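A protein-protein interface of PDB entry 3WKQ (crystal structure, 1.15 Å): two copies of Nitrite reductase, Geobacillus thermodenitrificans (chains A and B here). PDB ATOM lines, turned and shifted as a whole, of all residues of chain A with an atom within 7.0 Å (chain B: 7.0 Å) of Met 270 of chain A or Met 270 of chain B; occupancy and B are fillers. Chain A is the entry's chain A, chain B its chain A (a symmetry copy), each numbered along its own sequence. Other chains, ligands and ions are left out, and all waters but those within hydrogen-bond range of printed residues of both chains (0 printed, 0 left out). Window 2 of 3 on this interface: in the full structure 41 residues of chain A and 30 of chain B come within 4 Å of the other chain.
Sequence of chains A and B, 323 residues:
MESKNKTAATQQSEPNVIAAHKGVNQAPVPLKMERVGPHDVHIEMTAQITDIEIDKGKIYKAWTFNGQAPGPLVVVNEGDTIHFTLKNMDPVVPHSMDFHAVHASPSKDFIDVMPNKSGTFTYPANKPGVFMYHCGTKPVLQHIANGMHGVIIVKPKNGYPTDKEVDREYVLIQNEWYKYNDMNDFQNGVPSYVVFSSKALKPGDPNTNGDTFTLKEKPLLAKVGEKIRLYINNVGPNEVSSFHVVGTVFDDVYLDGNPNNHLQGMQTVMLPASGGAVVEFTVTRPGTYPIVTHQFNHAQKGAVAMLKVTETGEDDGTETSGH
CG1 of Val 240 of chain A touches CG2 of Val 240 of chain B, at 3.9 Å. CE of Met 270 of chain B touches CG1 of Val 240 of chain A (3.9 Å). Met 270 of chain B touches Met 270 of chain A (CG to CG, 3.99 Å). Pro 272 of chain A touches Ser 242 of chain B. CG of Pro 272 of chain A touches CG2 of Thr 268 of chain B (3.8 Å). Met 270 of chain B touches Pro 272 of chain A (SD to CA, 3.6 Å). Thr 268 of chain B touches Ala 273 of chain A (CG2 to O, 3.7 Å). CB of Ala 273 of chain A touches CG of Gln 295 of chain B, at 3.8 Å.
Val 240 of chain A touches its own counterpart, Val 240 of chain B. Val 240 of chain A touches Met 270 of chain B, but with the chains exchanged Met 270 of chain A does not touch Val 240 of chain B (6.7 Å). Pro 272 of chain A touches Thr 268 of chain B, but with the chains exchanged Thr 268 of chain A does not touch Pro 272 of chain B (14.0 Å). Pro 272 of chain A touches Met 270 of chain B, but with the chains exchanged Met 270 of chain A does not touch Pro 272 of chain B (7.9 Å). 15 positions are printed for both chains. Of the 9 pairs that touch across the chains among the printed residues, 2 have their exchanged pair printed and touching as well.
OE1 of Gln 295 of chain B lies within hydrogen-bond range of OG of Ser 242 of chain B (2.7 Å). O of Val 240 of chain A sits at hydrogen-bond distance from NE2 of Gln 295 of chain A, 3.1 Å away. The backbone carbonyl oxygen of Val 240 of chain B is in hydrogen-bond range of the side-chain amide nitrogen of Gln 295 of chain B, at 3.1 Å.
Of the printed residues of chain B, Met 270 of chain A touches Met 270 (3.99 Å). Of the printed residues of chain B, Pro 272 of chain A touches Ser 242 (3.3 Å), Thr 268 (3.8 Å) and Met 270 (3.6 Å). Printed residues of chain A within 4 Å of Val 240 of chain B: Val 240. Of the printed residues of chain A, Ser 242 of chain B touches Pro 272 and Ala 273. Of the printed residues of chain A, Met 270 of chain B touches Val 240, Met 270 and Pro 272. The nearest printed residue of chain B that does not touch Met 270 of chain A is Val 240 of chain B (6.7 Å).
The backbone NH (N) of Ala 273 of chain A lies within hydrogen-bond range of the side-chain hydroxyl (OG) of Ser 242 of chain B, 3.0 Å away.
Hydrophobic or aromatic side chains of chain A within 4 Å of the printed part of chain B: Val 240, Met 270, Pro 272 and Ala 273. Of the 15 printed residues of chain B, 5 touch a printed residue of chain A. Hydrophobic or aromatic side chains of chain B that line the printed part of chain A: Val 240 and Met 270. Among the printed residues, 9 pairs touch across the chains. Among the printed residues, no Asp or Glu carboxylate lies within 4 Å of a Lys or Arg side-chain nitrogen of the other chain.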
ATOM      1  N   VAL A 240      -9.241   3.680  20.440  1.00  0.00           N
ATOM      2  CA  VAL A 240      -9.296   5.109  20.304  1.00  0.00           C
ATOM      3  C   VAL A 240      -7.978   5.607  19.744  1.00  0.00           C
ATOM      4  O   VAL A 240      -6.967   4.861  19.721  1.00  0.00           O
ATOM      5  CB  VAL A 240      -9.700   5.781  21.632  1.00  0.00           C
ATOM      6  CG1 VAL A 240     -11.025   5.218  22.121  1.00  0.00           C
ATOM      7  CG2 VAL A 240      -8.586   5.641  22.680  1.00  0.00           C
ATOM      8  N   SER A 241      -7.949   6.857  19.278  1.00  0.00           N
ATOM      9  CA  SER A 241      -6.754   7.452  18.654  1.00  0.00           C
ATOM     10  C   SER A 241      -6.411   8.810  19.291  1.00  0.00           C
ATOM     11  O   SER A 241      -7.263   9.615  19.603  1.00  0.00           O
ATOM     12  CB  SER A 241      -6.975   7.618  17.134  1.00  0.00           C
ATOM     13  OG  SER A 241      -5.874   8.274  16.540  1.00  0.00           O
ATOM     14  N   SER A 242      -5.098   9.011  19.464  1.00  0.00           N
ATOM     15  CA  SER A 242      -4.555  10.247  20.062  1.00  0.00           C
ATOM     16  C   SER A 242      -3.764  10.984  18.939  1.00  0.00           C
ATOM     17  O   SER A 242      -2.594  10.820  18.784  1.00  0.00           O
ATOM     18  CB  SER A 242      -3.655   9.879  21.242  1.00  0.00           C
ATOM     19  OG  SER A 242      -4.425   9.267  22.276  1.00  0.00           O
ATOM     20  N   PHE A 243      -4.523  11.654  18.062  1.00  0.00           N
ATOM     21  CA  PHE A 243      -3.974  12.051  16.792  1.00  0.00           C
ATOM     22  C   PHE A 243      -3.077  13.333  16.930  1.00  0.00           C
ATOM     23  O   PHE A 243      -3.493  14.321  17.501  1.00  0.00           O
ATOM     24  CB  PHE A 243      -5.107  12.325  15.822  1.00  0.00           C
ATOM     25  CG  PHE A 243      -4.653  12.623  14.434  1.00  0.00           C
ATOM     26  CD1 PHE A 243      -4.303  11.595  13.547  1.00  0.00           C
ATOM     27  CD2 PHE A 243      -4.461  13.955  14.001  1.00  0.00           C
ATOM     28  CE1 PHE A 243      -3.840  11.867  12.262  1.00  0.00           C
ATOM     29  CE2 PHE A 243      -3.991  14.229  12.698  1.00  0.00           C
ATOM     30  CZ  PHE A 243      -3.685  13.199  11.840  1.00  0.00           C
ATOM     31  N   LEU A 255     -14.554  19.090  15.768  1.00  0.00           N
ATOM     32  CA  LEU A 255     -14.837  17.703  16.134  1.00  0.00           C
ATOM     33  C   LEU A 255     -15.973  17.161  15.233  1.00  0.00           C
ATOM     34  O   LEU A 255     -17.019  17.828  15.015  1.00  0.00           O
ATOM     35  CB  LEU A 255     -15.254  17.543  17.609  1.00  0.00           C
ATOM     36  CG  LEU A 255     -14.181  18.043  18.629  1.00  0.00           C
ATOM     37  CD1 LEU A 255     -14.732  17.845  20.040  1.00  0.00           C
ATOM     38  CD2 LEU A 255     -12.869  17.278  18.477  1.00  0.00           C
ATOM     39  N   MET A 266      -4.728  22.825  19.770  1.00  0.00           N
ATOM     40  CA  MET A 266      -4.632  21.474  20.353  1.00  0.00           C
ATOM     41  C   MET A 266      -3.348  20.852  19.907  1.00  0.00           C
ATOM     42  O   MET A 266      -3.004  20.871  18.717  1.00  0.00           O
ATOM     43  CB  MET A 266      -5.812  20.624  19.917  1.00  0.00           C
ATOM     44  CG  MET A 266      -7.185  21.078  20.356  1.00  0.00           C
ATOM     45  SD  MET A 266      -7.520  21.021  22.128  1.00  0.00           S
ATOM     46  CE  MET A 266      -7.523  19.250  22.468  1.00  0.00           C
ATOM     47  N   THR A 268      -3.003  17.496  20.354  1.00  0.00           N
ATOM     48  CA  THR A 268      -3.355  16.136  20.069  1.00  0.00           C
ATOM     49  C   THR A 268      -4.875  16.052  20.169  1.00  0.00           C
ATOM     50  O   THR A 268      -5.492  16.647  21.071  1.00  0.00           O
ATOM     51  CB  THR A 268      -2.747  15.159  21.134  1.00  0.00           C
ATOM     52  OG1 THR A 268      -1.316  15.274  20.893  1.00  0.00           O
ATOM     53  CG2 THR A 268      -3.217  13.735  20.940  1.00  0.00           C
ATOM     54  N   VAL A 269      -5.529  15.363  19.196  1.00  0.00           N
ATOM     55  CA  VAL A 269      -6.984  15.279  19.168  1.00  0.00           C
ATOM     56  C   VAL A 269      -7.383  13.815  19.524  1.00  0.00           C
ATOM     57  O   VAL A 269      -7.022  12.876  18.830  1.00  0.00           O
ATOM     58  CB  VAL A 269      -7.503  15.657  17.784  1.00  0.00           C
ATOM     59  CG1 VAL A 269      -9.011  15.457  17.703  1.00  0.00           C
ATOM     60  CG2 VAL A 269      -7.155  17.119  17.519  1.00  0.00           C
ATOM     61  N   MET A 270      -8.183  13.698  20.574  1.00  0.00           N
ATOM     62  CA  MET A 270      -8.712  12.390  21.032  1.00  0.00           C
ATOM     63  C   MET A 270      -9.862  11.987  20.107  1.00  0.00           C
ATOM     64  O   MET A 270     -10.866  12.711  20.060  1.00  0.00           O
ATOM     65  CB  MET A 270      -9.181  12.601  22.485  1.00  0.00           C
ATOM     66  CG  MET A 270      -9.853  11.473  23.193  1.00  0.00           C
ATOM     67  SD  MET A 270      -8.772  10.271  23.906  1.00  0.00           S
ATOM     68  CE  MET A 270      -8.294   9.247  22.519  1.00  0.00           C
ATOM     69  N   LEU A 271      -9.773  10.859  19.442  1.00  0.00           N
ATOM     70  CA  LEU A 271     -10.836  10.362  18.586  1.00  0.00           C
ATOM     71  C   LEU A 271     -11.374   9.067  19.154  1.00  0.00           C
ATOM     72  O   LEU A 271     -10.598   8.118  19.329  1.00  0.00           O
ATOM     73  CB  LEU A 271     -10.352  10.048  17.169  1.00  0.00           C
ATOM     74  CG  LEU A 271      -9.742  11.262  16.418  1.00  0.00           C
ATOM     75  CD1 LEU A 271      -9.147  10.781  15.166  1.00  0.00           C
ATOM     76  CD2 LEU A 271     -10.840  12.344  16.110  1.00  0.00           C
ATOM     77  N   PRO A 272     -12.682   8.967  19.449  1.00  0.00           N
ATOM     78  CA  PRO A 272     -13.260   7.673  19.774  1.00  0.00           C
ATOM     79  C   PRO A 272     -13.138   6.723  18.585  1.00  0.00           C
ATOM     80  O   PRO A 272     -12.819   7.156  17.464  1.00  0.00           O
ATOM     81  CB  PRO A 272     -14.717   8.021  20.133  1.00  0.00           C
ATOM     82  CG  PRO A 272     -15.009   9.266  19.329  1.00  0.00           C
ATOM     83  CD  PRO A 272     -13.701  10.013  19.268  1.00  0.00           C
ATOM     84  N   ALA A 273     -13.466   5.455  18.801  1.00  0.00           N
ATOM     85  CA  ALA A 273     -13.667   4.559  17.654  1.00  0.00           C
ATOM     86  C   ALA A 273     -14.864   5.073  16.858  1.00  0.00           C
ATOM     87  O   ALA A 273     -15.919   5.299  17.466  1.00  0.00           O
ATOM     88  CB  ALA A 273     -13.912   3.144  18.159  1.00  0.00           C
ATOM     89  N   GLY A 275     -14.666   8.004  15.483  1.00  0.00           N
ATOM     90  CA  GLY A 275     -14.596   9.461  15.627  1.00  0.00           C
ATOM     91  C   GLY A 275     -13.857  10.111  14.455  1.00  0.00           C
ATOM     92  O   GLY A 275     -12.822   9.648  13.995  1.00  0.00           O
ATOM     93  N   GLY A 276     -14.378  11.281  14.083  1.00  0.00           N
ATOM     94  CA  GLY A 276     -13.778  12.103  13.047  1.00  0.00           C
ATOM     95  C   GLY A 276     -13.387  13.484  13.508  1.00  0.00           C
ATOM     96  O   GLY A 276     -13.786  13.936  14.588  1.00  0.00           O
ATOM     97  N   ALA A 277     -12.658  14.186  12.653  1.00  0.00           N
ATOM     98  CA  ALA A 277     -12.345  15.565  12.896  1.00  0.00           C
ATOM     99  C   ALA A 277     -11.897  16.190  11.595  1.00  0.00           C
ATOM    100  O   ALA A 277     -11.400  15.512  10.696  1.00  0.00           O
ATOM    101  CB  ALA A 277     -11.262  15.761  13.962  1.00  0.00           C
ATOM    102  N   GLN A 295      -0.611   7.139  21.041  1.00  0.00           N
ATOM    103  CA  GLN A 295      -0.581   5.845  21.790  1.00  0.00           C
ATOM    104  C   GLN A 295       0.519   5.054  21.092  1.00  0.00           C
ATOM    105  O   GLN A 295       0.342   4.480  20.050  1.00  0.00           O
ATOM    106  CB  GLN A 295      -1.954   5.206  21.712  1.00  0.00           C
ATOM    107  CG  GLN A 295      -2.976   6.011  22.513  1.00  0.00           C
ATOM    108  CD  GLN A 295      -4.429   5.796  22.008  1.00  0.00           C
ATOM    109  OE1 GLN A 295      -5.090   6.723  21.645  1.00  0.00           O
ATOM    110  NE2 GLN A 295      -4.869   4.523  21.972  1.00  0.00           N
ATOM    111  N   VAL B 240     -12.960   3.191  28.352  1.00  0.00           N
ATOM    112  CA  VAL B 240     -13.639   4.324  27.785  1.00  0.00           C
ATOM    113  C   VAL B 240     -14.723   3.837  26.846  1.00  0.00           C
ATOM    114  O   VAL B 240     -14.749   2.642  26.459  1.00  0.00           O
ATOM    115  CB  VAL B 240     -12.642   5.302  27.131  1.00  0.00           C
ATOM    116  CG1 VAL B 240     -11.590   5.731  28.141  1.00  0.00           C
ATOM    117  CG2 VAL B 240     -12.019   4.688  25.868  1.00  0.00           C
ATOM    118  N   SER B 241     -15.640   4.727  26.461  1.00  0.00           N
ATOM    119  CA  SER B 241     -16.781   4.381  25.597  1.00  0.00           C
ATOM    120  C   SER B 241     -16.885   5.340  24.398  1.00  0.00           C
ATOM    121  O   SER B 241     -16.683   6.531  24.502  1.00  0.00           O
ATOM    122  CB  SER B 241     -18.093   4.405  26.414  1.00  0.00           C
ATOM    123  OG  SER B 241     -19.205   4.167  25.576  1.00  0.00           O
ATOM    124  N   SER B 242     -17.216   4.738  23.249  1.00  0.00           N
ATOM    125  CA  SER B 242     -17.365   5.476  21.978  1.00  0.00           C
ATOM    126  C   SER B 242     -18.872   5.404  21.588  1.00  0.00           C
ATOM    127  O   SER B 242     -19.295   4.549  20.873  1.00  0.00           O
ATOM    128  CB  SER B 242     -16.471   4.833  20.918  1.00  0.00           C
ATOM    129  OG  SER B 242     -15.098   4.975  21.279  1.00  0.00           O
ATOM    130  N   PHE B 243     -19.669   6.247  22.256  1.00  0.00           N
ATOM    131  CA  PHE B 243     -21.092   6.031  22.274  1.00  0.00           C
ATOM    132  C   PHE B 243     -21.764   6.521  20.942  1.00  0.00           C
ATOM    133  O   PHE B 243     -21.545   7.635  20.510  1.00  0.00           O
ATOM    134  CB  PHE B 243     -21.695   6.774  23.450  1.00  0.00           C
ATOM    135  CG  PHE B 243     -23.151   6.518  23.642  1.00  0.00           C
ATOM    136  CD1 PHE B 243     -23.607   5.362  24.293  1.00  0.00           C
ATOM    137  CD2 PHE B 243     -24.121   7.380  23.083  1.00  0.00           C
ATOM    138  CE1 PHE B 243     -24.966   5.097  24.440  1.00  0.00           C
ATOM    139  CE2 PHE B 243     -25.499   7.110  23.232  1.00  0.00           C
ATOM    140  CZ  PHE B 243     -25.916   5.984  23.902  1.00  0.00           C
ATOM    141  N   LEU B 255     -21.606  17.739  27.292  1.00  0.00           N
ATOM    142  CA  LEU B 255     -20.644  16.877  27.978  1.00  0.00           C
ATOM    143  C   LEU B 255     -20.857  16.992  29.507  1.00  0.00           C
ATOM    144  O   LEU B 255     -20.997  18.109  30.073  1.00  0.00           O
ATOM    145  CB  LEU B 255     -19.180  17.233  27.653  1.00  0.00           C
ATOM    146  CG  LEU B 255     -18.828  17.142  26.132  1.00  0.00           C
ATOM    147  CD1 LEU B 255     -17.364  17.537  25.954  1.00  0.00           C
ATOM    148  CD2 LEU B 255     -19.049  15.731  25.594  1.00  0.00           C
ATOM    149  N   MET B 266     -22.650  15.404  16.339  1.00  0.00           N
ATOM    150  CA  MET B 266     -21.630  14.378  16.622  1.00  0.00           C
ATOM    151  C   MET B 266     -22.154  13.050  16.179  1.00  0.00           C
ATOM    152  O   MET B 266     -23.292  12.672  16.487  1.00  0.00           O
ATOM    153  CB  MET B 266     -21.304  14.351  18.105  1.00  0.00           C
ATOM    154  CG  MET B 266     -20.691  15.599  18.697  1.00  0.00           C
ATOM    155  SD  MET B 266     -19.038  16.032  18.120  1.00  0.00           S
ATOM    156  CE  MET B 266     -18.028  14.697  18.790  1.00  0.00           C
ATOM    157  N   THR B 268     -20.515  10.280  17.284  1.00  0.00           N
ATOM    158  CA  THR B 268     -20.104   9.378  18.321  1.00  0.00           C
ATOM    159  C   THR B 268     -19.522  10.240  19.438  1.00  0.00           C
ATOM    160  O   THR B 268     -18.798  11.218  19.181  1.00  0.00           O
ATOM    161  CB  THR B 268     -18.975   8.414  17.818  1.00  0.00           C
ATOM    162  OG1 THR B 268     -19.665   7.608  16.821  1.00  0.00           O
ATOM    163  CG2 THR B 268     -18.425   7.548  18.928  1.00  0.00           C
ATOM    164  N   VAL B 269     -19.884   9.939  20.713  1.00  0.00           N
ATOM    165  CA  VAL B 269     -19.433  10.741  21.844  1.00  0.00           C
ATOM    166  C   VAL B 269     -18.412   9.887  22.655  1.00  0.00           C
ATOM    167  O   VAL B 269     -18.741   8.825  23.162  1.00  0.00           O
ATOM    168  CB  VAL B 269     -20.622  11.133  22.715  1.00  0.00           C
ATOM    169  CG1 VAL B 269     -20.152  11.867  23.965  1.00  0.00           C
ATOM    170  CG2 VAL B 269     -21.547  12.030  21.899  1.00  0.00           C
ATOM    171  N   MET B 270     -17.216  10.440  22.798  1.00  0.00           N
ATOM    172  CA  MET B 270     -16.131   9.802  23.584  1.00  0.00           C
ATOM    173  C   MET B 270     -16.416  10.031  25.068  1.00  0.00           C
ATOM    174  O   MET B 270     -16.445  11.193  25.494  1.00  0.00           O
ATOM    175  CB  MET B 270     -14.821  10.476  23.132  1.00  0.00           C
ATOM    176  CG  MET B 270     -13.550  10.105  23.819  1.00  0.00           C
ATOM    177  SD  MET B 270     -12.777   8.625  23.241  1.00  0.00           S
ATOM    178  CE  MET B 270     -13.705   7.317  24.035  1.00  0.00           C
ATOM    179  N   LEU B 271     -16.562   8.988  25.852  1.00  0.00           N
ATOM    180  CA  LEU B 271     -16.776   9.102  27.285  1.00  0.00           C
ATOM    181  C   LEU B 271     -15.600   8.496  28.018  1.00  0.00           C
ATOM    182  O   LEU B 271     -15.300   7.313  27.805  1.00  0.00           O
ATOM    183  CB  LEU B 271     -18.018   8.343  27.756  1.00  0.00           C
ATOM    184  CG  LEU B 271     -19.343   8.812  27.095  1.00  0.00           C
ATOM    185  CD1 LEU B 271     -20.409   7.882  27.482  1.00  0.00           C
ATOM    186  CD2 LEU B 271     -19.712  10.272  27.547  1.00  0.00           C
ATOM    187  N   PRO B 272     -14.907   9.249  28.892  1.00  0.00           N
ATOM    188  CA  PRO B 272     -13.928   8.631  29.771  1.00  0.00           C
ATOM    189  C   PRO B 272     -14.605   7.625  30.699  1.00  0.00           C
ATOM    190  O   PRO B 272     -15.845   7.598  30.799  1.00  0.00           O
ATOM    191  CB  PRO B 272     -13.315   9.834  30.514  1.00  0.00           C
ATOM    192  CG  PRO B 272     -14.424  10.860  30.532  1.00  0.00           C
ATOM    193  CD  PRO B 272     -15.176  10.652  29.241  1.00  0.00           C
ATOM    194  N   GLY B 275     -17.336   9.062  32.720  1.00  0.00           N
ATOM    195  CA  GLY B 275     -17.822  10.185  31.915  1.00  0.00           C
ATOM    196  C   GLY B 275     -19.320  10.069  31.626  1.00  0.00           C
ATOM    197  O   GLY B 275     -19.845   9.013  31.298  1.00  0.00           O
ATOM    198  N   GLY B 276     -19.956  11.241  31.641  1.00  0.00           N
ATOM    199  CA  GLY B 276     -21.364  11.365  31.309  1.00  0.00           C
ATOM    200  C   GLY B 276     -21.644  12.287  30.149  1.00  0.00           C
ATOM    201  O   GLY B 276     -20.774  13.049  29.713  1.00  0.00           O
ATOM    202  N   ALA B 277     -22.887  12.266  29.691  1.00  0.00           N
ATOM    203  CA  ALA B 277     -23.330  13.199  28.694  1.00  0.00           C
ATOM    204  C   ALA B 277     -24.841  13.217  28.695  1.00  0.00           C
ATOM    205  O   ALA B 277     -25.493  12.246  29.078  1.00  0.00           O
ATOM    206  CB  ALA B 277     -22.818  12.870  27.288  1.00  0.00           C
ATOM    207  N   GLN B 295     -16.463   0.825  20.049  1.00  0.00           N
ATOM    208  CA  GLN B 295     -15.302  -0.091  20.274  1.00  0.00           C
ATOM    209  C   GLN B 295     -15.919  -1.481  20.166  1.00  0.00           C
ATOM    210  O   GLN B 295     -16.532  -1.989  21.068  1.00  0.00           O
ATOM    211  CB  GLN B 295     -14.694   0.218  21.627  1.00  0.00           C
ATOM    212  CG  GLN B 295     -14.018   1.588  21.622  1.00  0.00           C
ATOM    213  CD  GLN B 295     -13.925   2.211  23.041  1.00  0.00           C
ATOM    214  OE1 GLN B 295     -14.412   3.279  23.270  1.00  0.00           O
ATOM    215  NE2 GLN B 295     -13.308   1.470  23.982  1.00  0.00           N
